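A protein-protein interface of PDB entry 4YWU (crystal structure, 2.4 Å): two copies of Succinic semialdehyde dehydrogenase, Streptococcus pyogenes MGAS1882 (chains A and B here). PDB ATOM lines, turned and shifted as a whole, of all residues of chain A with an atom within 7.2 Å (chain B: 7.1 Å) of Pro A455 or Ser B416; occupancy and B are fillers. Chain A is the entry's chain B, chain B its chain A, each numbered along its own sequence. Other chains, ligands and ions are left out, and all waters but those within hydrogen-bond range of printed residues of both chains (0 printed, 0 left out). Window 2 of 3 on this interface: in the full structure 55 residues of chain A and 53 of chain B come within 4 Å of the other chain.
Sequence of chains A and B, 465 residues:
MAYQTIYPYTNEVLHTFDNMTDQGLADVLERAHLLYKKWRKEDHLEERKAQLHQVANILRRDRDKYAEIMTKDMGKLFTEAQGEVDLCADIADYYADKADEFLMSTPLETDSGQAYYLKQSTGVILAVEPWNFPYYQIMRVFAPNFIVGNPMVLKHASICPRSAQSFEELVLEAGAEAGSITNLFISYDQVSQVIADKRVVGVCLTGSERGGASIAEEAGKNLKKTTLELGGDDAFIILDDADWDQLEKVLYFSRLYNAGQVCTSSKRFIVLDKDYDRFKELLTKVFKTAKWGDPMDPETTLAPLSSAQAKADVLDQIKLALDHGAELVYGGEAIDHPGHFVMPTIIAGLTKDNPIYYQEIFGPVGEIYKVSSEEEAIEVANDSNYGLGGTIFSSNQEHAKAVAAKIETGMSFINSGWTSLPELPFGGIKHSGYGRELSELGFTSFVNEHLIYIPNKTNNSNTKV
The side-chain amide nitrogen (NE2) of Gln B397 is in hydrogen-bond range of the side-chain amide oxygen (OE1) of Gln A114 (3.3 Å). The backbone carbonyl oxygen (O) of Ser B412 lies within hydrogen-bond range of the backbone NH (N) of Tyr A453, 2.9 Å away. The backbone carbonyl oxygen of Tyr A453 sits at hydrogen-bond distance from the backbone NH of Ile B414, 3.0 Å away.
No position is printed for both chains.
Phe B413 touches Tyr A453 (CA to O, 3.7 Å). CE2 of Tyr A453 touches OG1 of Thr B419, 3.7 Å away. Ile A454 touches Ile B414. CD of Pro A455 touches O of Ile B414, at 3.7 Å. CG of Pro A455 touches OG of Ser B416, 3.6 Å away.
The backbone NH (N) of Phe B413 is in hydrogen-bond range of the backbone carbonyl oxygen (O) of Gly B390 (2.8 Å). The side-chain hydroxyl (OG1) of Thr B391 lies within hydrogen-bond range of the backbone carbonyl oxygen (O) of Ser B416. N of Ile B392 lies within hydrogen-bond range of O of Phe B413 (2.9 Å). The backbone carbonyl oxygen (O) of Ile B414 lies within hydrogen-bond range of the side-chain hydroxyl (OG) of Ser B416, 3.1 Å away. OH of Tyr A453 sits close to O of Ser A112. O of Gln A114 lies within hydrogen-bond range of N of Ile A454 (2.9 Å).
Of the 9 printed residues of chain A, 4 touch a printed residue of chain B. Hydrophobic or aromatic side chains of chain A that line the printed part of chain B: Tyr A453, Ile A454 and Pro A455. Printed residues of chain B that touch a printed residue of chain A: Gln B397, Ser B412, Phe B413, Ile B414, Ser B416 and Thr B419. Hydrophobic or aromatic side chains of chain B within 4 Å of the printed part of chain A: Ile B414. Among the printed residues, no Asp or Glu carboxylate lies within 4 Å of a Lys or Arg side-chain nitrogen of the other chain.
Of the printed residues of chain B, Tyr A453 touches Ser B412, Phe B413, Ile B414 and Thr B419. Of the printed residues of chain B, Ile A454 touches Ile B414 (3.5 Å). Of the printed residues of chain B, Pro A455 touches Ile B414 and Ser B416. Thr B391 touches none of the printed residues of chain A. Of the printed residues of chain A, Ser B412 touches Tyr A453. Ser B416 touches one residue of chain A. The nearest residue of chain B that does not touch Pro A455 is Asn B415 (5.1 Å). The nearest residue of chain A that does not touch Ser B416 is Tyr A453 (5.1 Å).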
ATOM      1  N   ASP A 111     -28.377  12.561  27.768  1.00  0.00           N
ATOM      2  CA  ASP A 111     -28.172  13.944  28.195  1.00  0.00           C
ATOM      3  C   ASP A 111     -27.778  14.742  26.961  1.00  0.00           C
ATOM      4  O   ASP A 111     -27.973  15.955  26.887  1.00  0.00           O
ATOM      5  CB  ASP A 111     -27.029  14.046  29.216  1.00  0.00           C
ATOM      6  CG  ASP A 111     -26.818  12.763  30.002  1.00  0.00           C
ATOM      7  OD1 ASP A 111     -26.491  11.728  29.374  1.00  0.00           O
ATOM      8  OD2 ASP A 111     -26.972  12.791  31.246  1.00  0.00           O
ATOM      9  N   SER A 112     -27.215  14.032  25.993  1.00  0.00           N
ATOM     10  CA  SER A 112     -26.747  14.631  24.756  1.00  0.00           C
ATOM     11  C   SER A 112     -27.845  15.241  23.896  1.00  0.00           C
ATOM     12  O   SER A 112     -27.558  15.905  22.902  1.00  0.00           O
ATOM     13  CB  SER A 112     -25.986  13.580  23.955  1.00  0.00           C
ATOM     14  OG  SER A 112     -25.002  12.955  24.765  1.00  0.00           O
ATOM     15  N   GLY A 113     -29.098  15.022  24.274  1.00  0.00           N
ATOM     16  CA  GLY A 113     -30.199  15.560  23.500  1.00  0.00           C
ATOM     17  C   GLY A 113     -31.412  14.652  23.523  1.00  0.00           C
ATOM     18  O   GLY A 113     -31.630  13.925  24.489  1.00  0.00           O
ATOM     19  N   GLN A 114     -32.204  14.680  22.457  1.00  0.00           N
ATOM     20  CA  GLN A 114     -33.404  13.853  22.391  1.00  0.00           C
ATOM     21  C   GLN A 114     -33.207  12.703  21.419  1.00  0.00           C
ATOM     22  O   GLN A 114     -32.649  12.879  20.340  1.00  0.00           O
ATOM     23  CB  GLN A 114     -34.606  14.703  21.960  1.00  0.00           C
ATOM     24  CG  GLN A 114     -34.748  16.005  22.753  1.00  0.00           C
ATOM     25  CD  GLN A 114     -35.899  16.876  22.271  1.00  0.00           C
ATOM     26  OE1 GLN A 114     -36.032  17.148  21.072  1.00  0.00           O
ATOM     27  NE2 GLN A 114     -36.732  17.331  23.208  1.00  0.00           N
ATOM     28  N   ALA A 115     -33.664  11.523  21.810  1.00  0.00           N
ATOM     29  CA  ALA A 115     -33.535  10.348  20.966  1.00  0.00           C
ATOM     30  C   ALA A 115     -34.683   9.373  21.198  1.00  0.00           C
ATOM     31  O   ALA A 115     -35.326   9.379  22.247  1.00  0.00           O
ATOM     32  CB  ALA A 115     -32.201   9.660  21.234  1.00  0.00           C
ATOM     33  N   TYR A 453     -31.771  10.523  16.235  1.00  0.00           N
ATOM     34  CA  TYR A 453     -31.013  11.225  17.260  1.00  0.00           C
ATOM     35  C   TYR A 453     -30.875  12.717  16.964  1.00  0.00           C
ATOM     36  O   TYR A 453     -30.514  13.123  15.861  1.00  0.00           O
ATOM     37  CB  TYR A 453     -29.625  10.594  17.417  1.00  0.00           C
ATOM     38  CG  TYR A 453     -28.735  11.297  18.425  1.00  0.00           C
ATOM     39  CD1 TYR A 453     -29.040  11.291  19.791  1.00  0.00           C
ATOM     40  CD2 TYR A 453     -27.600  11.986  18.010  1.00  0.00           C
ATOM     41  CE1 TYR A 453     -28.232  11.959  20.713  1.00  0.00           C
ATOM     42  CE2 TYR A 453     -26.787  12.658  18.920  1.00  0.00           C
ATOM     43  CZ  TYR A 453     -27.107  12.644  20.267  1.00  0.00           C
ATOM     44  OH  TYR A 453     -26.309  13.343  21.147  1.00  0.00           O
ATOM     45  N   ILE A 454     -31.170  13.529  17.974  1.00  0.00           N
ATOM     46  CA  ILE A 454     -31.092  14.972  17.856  1.00  0.00           C
ATOM     47  C   ILE A 454     -30.258  15.521  19.013  1.00  0.00           C
ATOM     48  O   ILE A 454     -30.732  15.605  20.148  1.00  0.00           O
ATOM     49  CB  ILE A 454     -32.503  15.594  17.913  1.00  0.00           C
ATOM     50  CG1 ILE A 454     -33.440  14.852  16.959  1.00  0.00           C
ATOM     51  CG2 ILE A 454     -32.441  17.055  17.526  1.00  0.00           C
ATOM     52  CD1 ILE A 454     -34.903  15.231  17.115  1.00  0.00           C
ATOM     53  N   PRO A 455     -28.988  15.864  18.751  1.00  0.00           N
ATOM     54  CA  PRO A 455     -28.139  16.403  19.820  1.00  0.00           C
ATOM     55  C   PRO A 455     -28.485  17.865  20.132  1.00  0.00           C
ATOM     56  O   PRO A 455     -29.304  18.476  19.440  1.00  0.00           O
ATOM     57  CB  PRO A 455     -26.727  16.218  19.262  1.00  0.00           C
ATOM     58  CG  PRO A 455     -26.932  16.336  17.790  1.00  0.00           C
ATOM     59  CD  PRO A 455     -28.193  15.546  17.554  1.00  0.00           C
ATOM     60  N   ASN A 456     -27.869  18.425  21.171  1.00  0.00           N
ATOM     61  CA  ASN A 456     -28.144  19.811  21.560  1.00  0.00           C
ATOM     62  C   ASN A 456     -27.172  20.831  20.956  1.00  0.00           C
ATOM     63  O   ASN A 456     -26.045  20.431  20.585  1.00  0.00           O
ATOM     64  CB  ASN A 456     -28.133  19.936  23.086  1.00  0.00           C
ATOM     65  CG  ASN A 456     -29.125  19.000  23.758  1.00  0.00           C
ATOM     66  OD1 ASN A 456     -30.326  19.042  23.477  1.00  0.00           O
ATOM     67  ND2 ASN A 456     -28.626  18.146  24.655  1.00  0.00           N
ATOM     68  N   PHE B 236     -26.466  12.300   3.430  1.00  0.00           N
ATOM     69  CA  PHE B 236     -26.480  13.522   4.219  1.00  0.00           C
ATOM     70  C   PHE B 236     -27.391  14.447   3.405  1.00  0.00           C
ATOM     71  O   PHE B 236     -26.966  15.052   2.422  1.00  0.00           O
ATOM     72  CB  PHE B 236     -25.053  14.059   4.307  1.00  0.00           C
ATOM     73  CG  PHE B 236     -24.879  15.226   5.239  1.00  0.00           C
ATOM     74  CD1 PHE B 236     -25.434  16.469   4.943  1.00  0.00           C
ATOM     75  CD2 PHE B 236     -24.097  15.097   6.382  1.00  0.00           C
ATOM     76  CE1 PHE B 236     -25.207  17.568   5.765  1.00  0.00           C
ATOM     77  CE2 PHE B 236     -23.861  16.190   7.217  1.00  0.00           C
ATOM     78  CZ  PHE B 236     -24.416  17.429   6.906  1.00  0.00           C
ATOM     79  N   VAL B 250     -20.121  21.417  10.936  1.00  0.00           N
ATOM     80  CA  VAL B 250     -20.029  19.961  11.015  1.00  0.00           C
ATOM     81  C   VAL B 250     -19.432  19.251   9.805  1.00  0.00           C
ATOM     82  O   VAL B 250     -19.051  18.095   9.908  1.00  0.00           O
ATOM     83  CB  VAL B 250     -21.429  19.321  11.288  1.00  0.00           C
ATOM     84  CG1 VAL B 250     -22.089  19.985  12.490  1.00  0.00           C
ATOM     85  CG2 VAL B 250     -22.313  19.450  10.065  1.00  0.00           C
ATOM     86  N   PHE B 253     -15.865  17.203  10.023  1.00  0.00           N
ATOM     87  CA  PHE B 253     -16.045  15.992  10.801  1.00  0.00           C
ATOM     88  C   PHE B 253     -16.861  14.958  10.034  1.00  0.00           C
ATOM     89  O   PHE B 253     -16.504  13.782   9.988  1.00  0.00           O
ATOM     90  CB  PHE B 253     -16.771  16.310  12.108  1.00  0.00           C
ATOM     91  CG  PHE B 253     -17.290  15.093  12.814  1.00  0.00           C
ATOM     92  CD1 PHE B 253     -16.434  14.270  13.534  1.00  0.00           C
ATOM     93  CD2 PHE B 253     -18.636  14.741  12.717  1.00  0.00           C
ATOM     94  CE1 PHE B 253     -16.907  13.108  14.150  1.00  0.00           C
ATOM     95  CE2 PHE B 253     -19.121  13.583  13.327  1.00  0.00           C
ATOM     96  CZ  PHE B 253     -18.253  12.764  14.045  1.00  0.00           C
ATOM     97  N   SER B 254     -17.959  15.405   9.436  1.00  0.00           N
ATOM     98  CA  SER B 254     -18.857  14.508   8.719  1.00  0.00           C
ATOM     99  C   SER B 254     -18.247  13.594   7.676  1.00  0.00           C
ATOM    100  O   SER B 254     -18.743  12.486   7.463  1.00  0.00           O
ATOM    101  CB  SER B 254     -19.997  15.303   8.088  1.00  0.00           C
ATOM    102  OG  SER B 254     -20.903  15.739   9.090  1.00  0.00           O
ATOM    103  N   SER B 266     -20.324  10.487   6.289  1.00  0.00           N
ATOM    104  CA  SER B 266     -21.322  11.101   5.431  1.00  0.00           C
ATOM    105  C   SER B 266     -20.801  10.982   4.004  1.00  0.00           C
ATOM    106  O   SER B 266     -20.279  11.944   3.438  1.00  0.00           O
ATOM    107  CB  SER B 266     -21.511  12.567   5.826  1.00  0.00           C
ATOM    108  OG  SER B 266     -21.922  12.678   7.183  1.00  0.00           O
ATOM    109  N   GLY B 390     -27.118   8.039   8.460  1.00  0.00           N
ATOM    110  CA  GLY B 390     -27.549   9.096   7.572  1.00  0.00           C
ATOM    111  C   GLY B 390     -27.844  10.347   8.382  1.00  0.00           C
ATOM    112  O   GLY B 390     -28.045  10.272   9.599  1.00  0.00           O
ATOM    113  N   THR B 391     -27.868  11.492   7.711  1.00  0.00           N
ATOM    114  CA  THR B 391     -28.129  12.760   8.369  1.00  0.00           C
ATOM    115  C   THR B 391     -29.192  13.545   7.628  1.00  0.00           C
ATOM    116  O   THR B 391     -29.249  13.511   6.403  1.00  0.00           O
ATOM    117  CB  THR B 391     -26.855  13.635   8.412  1.00  0.00           C
ATOM    118  OG1 THR B 391     -25.901  13.058   9.309  1.00  0.00           O
ATOM    119  CG2 THR B 391     -27.189  15.054   8.862  1.00  0.00           C
ATOM    120  N   ILE B 392     -30.039  14.238   8.377  1.00  0.00           N
ATOM    121  CA  ILE B 392     -31.061  15.091   7.782  1.00  0.00           C
ATOM    122  C   ILE B 392     -30.773  16.475   8.343  1.00  0.00           C
ATOM    123  O   ILE B 392     -30.791  16.666   9.555  1.00  0.00           O
ATOM    124  CB  ILE B 392     -32.500  14.691   8.188  1.00  0.00           C
ATOM    125  CG1 ILE B 392     -32.825  13.278   7.706  1.00  0.00           C
ATOM    126  CG2 ILE B 392     -33.492  15.675   7.578  1.00  0.00           C
ATOM    127  CD1 ILE B 392     -32.772  13.112   6.203  1.00  0.00           C
ATOM    128  N   PHE B 393     -30.491  17.430   7.461  1.00  0.00           N
ATOM    129  CA  PHE B 393     -30.187  18.797   7.872  1.00  0.00           C
ATOM    130  C   PHE B 393     -31.335  19.742   7.557  1.00  0.00           C
ATOM    131  O   PHE B 393     -31.653  19.993   6.389  1.00  0.00           O
ATOM    132  CB  PHE B 393     -28.915  19.278   7.188  1.00  0.00           C
ATOM    133  CG  PHE B 393     -27.920  19.858   8.131  1.00  0.00           C
ATOM    134  CD1 PHE B 393     -28.102  21.133   8.655  1.00  0.00           C
ATOM    135  CD2 PHE B 393     -26.825  19.106   8.546  1.00  0.00           C
ATOM    136  CE1 PHE B 393     -27.209  21.654   9.582  1.00  0.00           C
ATOM    137  CE2 PHE B 393     -25.925  19.614   9.471  1.00  0.00           C
ATOM    138  CZ  PHE B 393     -26.118  20.893   9.993  1.00  0.00           C
ATOM    139  N   GLN B 397     -37.346  21.112  13.223  1.00  0.00           N
ATOM    140  CA  GLN B 397     -37.224  19.812  13.867  1.00  0.00           C
ATOM    141  C   GLN B 397     -38.271  18.799  13.403  1.00  0.00           C
ATOM    142  O   GLN B 397     -37.925  17.703  12.963  1.00  0.00           O
ATOM    143  CB  GLN B 397     -37.301  19.977  15.387  1.00  0.00           C
ATOM    144  CG  GLN B 397     -36.623  18.852  16.155  1.00  0.00           C
ATOM    145  CD  GLN B 397     -36.922  18.887  17.642  1.00  0.00           C
ATOM    146  OE1 GLN B 397     -38.063  18.669  18.064  1.00  0.00           O
ATOM    147  NE2 GLN B 397     -35.897  19.161  18.446  1.00  0.00           N
ATOM    148  N   SER B 412     -30.591   7.809  12.012  1.00  0.00           N
ATOM    149  CA  SER B 412     -30.743   9.129  11.401  1.00  0.00           C
ATOM    150  C   SER B 412     -30.265  10.192  12.378  1.00  0.00           C
ATOM    151  O   SER B 412     -30.743  10.268  13.516  1.00  0.00           O
ATOM    152  CB  SER B 412     -32.203   9.423  11.036  1.00  0.00           C
ATOM    153  OG  SER B 412     -32.577   8.788   9.829  1.00  0.00           O
ATOM    154  N   PHE B 413     -29.329  11.015  11.922  1.00  0.00           N
ATOM    155  CA  PHE B 413     -28.767  12.075  12.737  1.00  0.00           C
ATOM    156  C   PHE B 413     -29.258  13.415  12.244  1.00  0.00           C
ATOM    157  O   PHE B 413     -29.022  13.793  11.100  1.00  0.00           O
ATOM    158  CB  PHE B 413     -27.254  11.992  12.672  1.00  0.00           C
ATOM    159  CG  PHE B 413     -26.722  10.662  13.099  1.00  0.00           C
ATOM    160  CD1 PHE B 413     -26.781  10.273  14.435  1.00  0.00           C
ATOM    161  CD2 PHE B 413     -26.190   9.778  12.165  1.00  0.00           C
ATOM    162  CE1 PHE B 413     -26.318   9.023  14.836  1.00  0.00           C
ATOM    163  CE2 PHE B 413     -25.720   8.516  12.559  1.00  0.00           C
ATOM    164  CZ  PHE B 413     -25.786   8.141  13.897  1.00  0.00           C
ATOM    165  N   ILE B 414     -29.948  14.130  13.120  1.00  0.00           N
ATOM    166  CA  ILE B 414     -30.499  15.427  12.771  1.00  0.00           C
ATOM    167  C   ILE B 414     -29.486  16.546  13.005  1.00  0.00           C
ATOM    168  O   ILE B 414     -28.895  16.643  14.080  1.00  0.00           O
ATOM    169  CB  ILE B 414     -31.761  15.718  13.601  1.00  0.00           C
ATOM    170  CG1 ILE B 414     -32.684  14.489  13.612  1.00  0.00           C
ATOM    171  CG2 ILE B 414     -32.466  16.943  13.046  1.00  0.00           C
ATOM    172  CD1 ILE B 414     -33.223  14.085  12.263  1.00  0.00           C
ATOM    173  N   ASN B 415     -29.299  17.383  11.988  1.00  0.00           N
ATOM    174  CA  ASN B 415     -28.370  18.498  12.048  1.00  0.00           C
ATOM    175  C   ASN B 415     -27.007  18.140  12.623  1.00  0.00           C
ATOM    176  O   ASN B 415     -26.449  18.878  13.444  1.00  0.00           O
ATOM    177  CB  ASN B 415     -28.972  19.643  12.851  1.00  0.00           C
ATOM    178  CG  ASN B 415     -30.196  20.219  12.189  1.00  0.00           C
ATOM    179  OD1 ASN B 415     -30.181  20.523  10.998  1.00  0.00           O
ATOM    180  ND2 ASN B 415     -31.266  20.376  12.954  1.00  0.00           N
ATOM    181  N   SER B 416     -26.460  17.012  12.186  1.00  0.00           N
ATOM    182  CA  SER B 416     -25.160  16.604  12.677  1.00  0.00           C
ATOM    183  C   SER B 416     -24.633  15.369  11.966  1.00  0.00           C
ATOM    184  O   SER B 416     -25.371  14.677  11.268  1.00  0.00           O
ATOM    185  CB  SER B 416     -25.243  16.330  14.177  1.00  0.00           C
ATOM    186  OG  SER B 416     -26.180  15.301  14.445  1.00  0.00           O
ATOM    187  N   GLY B 417     -23.338  15.118  12.139  1.00  0.00           N
ATOM    188  CA  GLY B 417     -22.720  13.949  11.548  1.00  0.00           C
ATOM    189  C   GLY B 417     -23.046  12.777  12.451  1.00  0.00           C
ATOM    190  O   GLY B 417     -23.849  12.910  13.378  1.00  0.00           O
ATOM    191  N   TRP B 418     -22.433  11.629  12.207  1.00  0.00           N
ATOM    192  CA  TRP B 418     -22.722  10.466  13.032  1.00  0.00           C
ATOM    193  C   TRP B 418     -22.214  10.640  14.464  1.00  0.00           C
ATOM    194  O   TRP B 418     -21.250  11.364  14.719  1.00  0.00           O
ATOM    195  CB  TRP B 418     -22.092   9.210  12.426  1.00  0.00           C
ATOM    196  CG  TRP B 418     -20.643   9.093  12.730  1.00  0.00           C
ATOM    197  CD1 TRP B 418     -19.624   9.827  12.189  1.00  0.00           C
ATOM    198  CD2 TRP B 418     -20.048   8.234  13.705  1.00  0.00           C
ATOM    199  NE1 TRP B 418     -18.428   9.476  12.769  1.00  0.00           N
ATOM    200  CE2 TRP B 418     -18.658   8.500  13.703  1.00  0.00           C
ATOM    201  CE3 TRP B 418     -20.553   7.262  14.583  1.00  0.00           C
ATOM    202  CZ2 TRP B 418     -17.767   7.828  14.547  1.00  0.00           C
ATOM    203  CZ3 TRP B 418     -19.665   6.594  15.422  1.00  0.00           C
ATOM    204  CH2 TRP B 418     -18.288   6.882  15.397  1.00  0.00           C
ATOM    205  N   THR B 419     -22.885   9.976  15.397  1.00  0.00           N
ATOM    206  CA  THR B 419     -22.495  10.013  16.799  1.00  0.00           C
ATOM    207  C   THR B 419     -22.648   8.585  17.303  1.00  0.00           C
ATOM    208  O   THR B 419     -23.257   7.742  16.641  1.00  0.00           O
ATOM    209  CB  THR B 419     -23.420  10.921  17.650  1.00  0.00           C
ATOM    210  OG1 THR B 419     -23.673  12.148  16.954  1.00  0.00           O
ATOM    211  CG2 THR B 419     -22.756  11.248  18.985  1.00  0.00           C
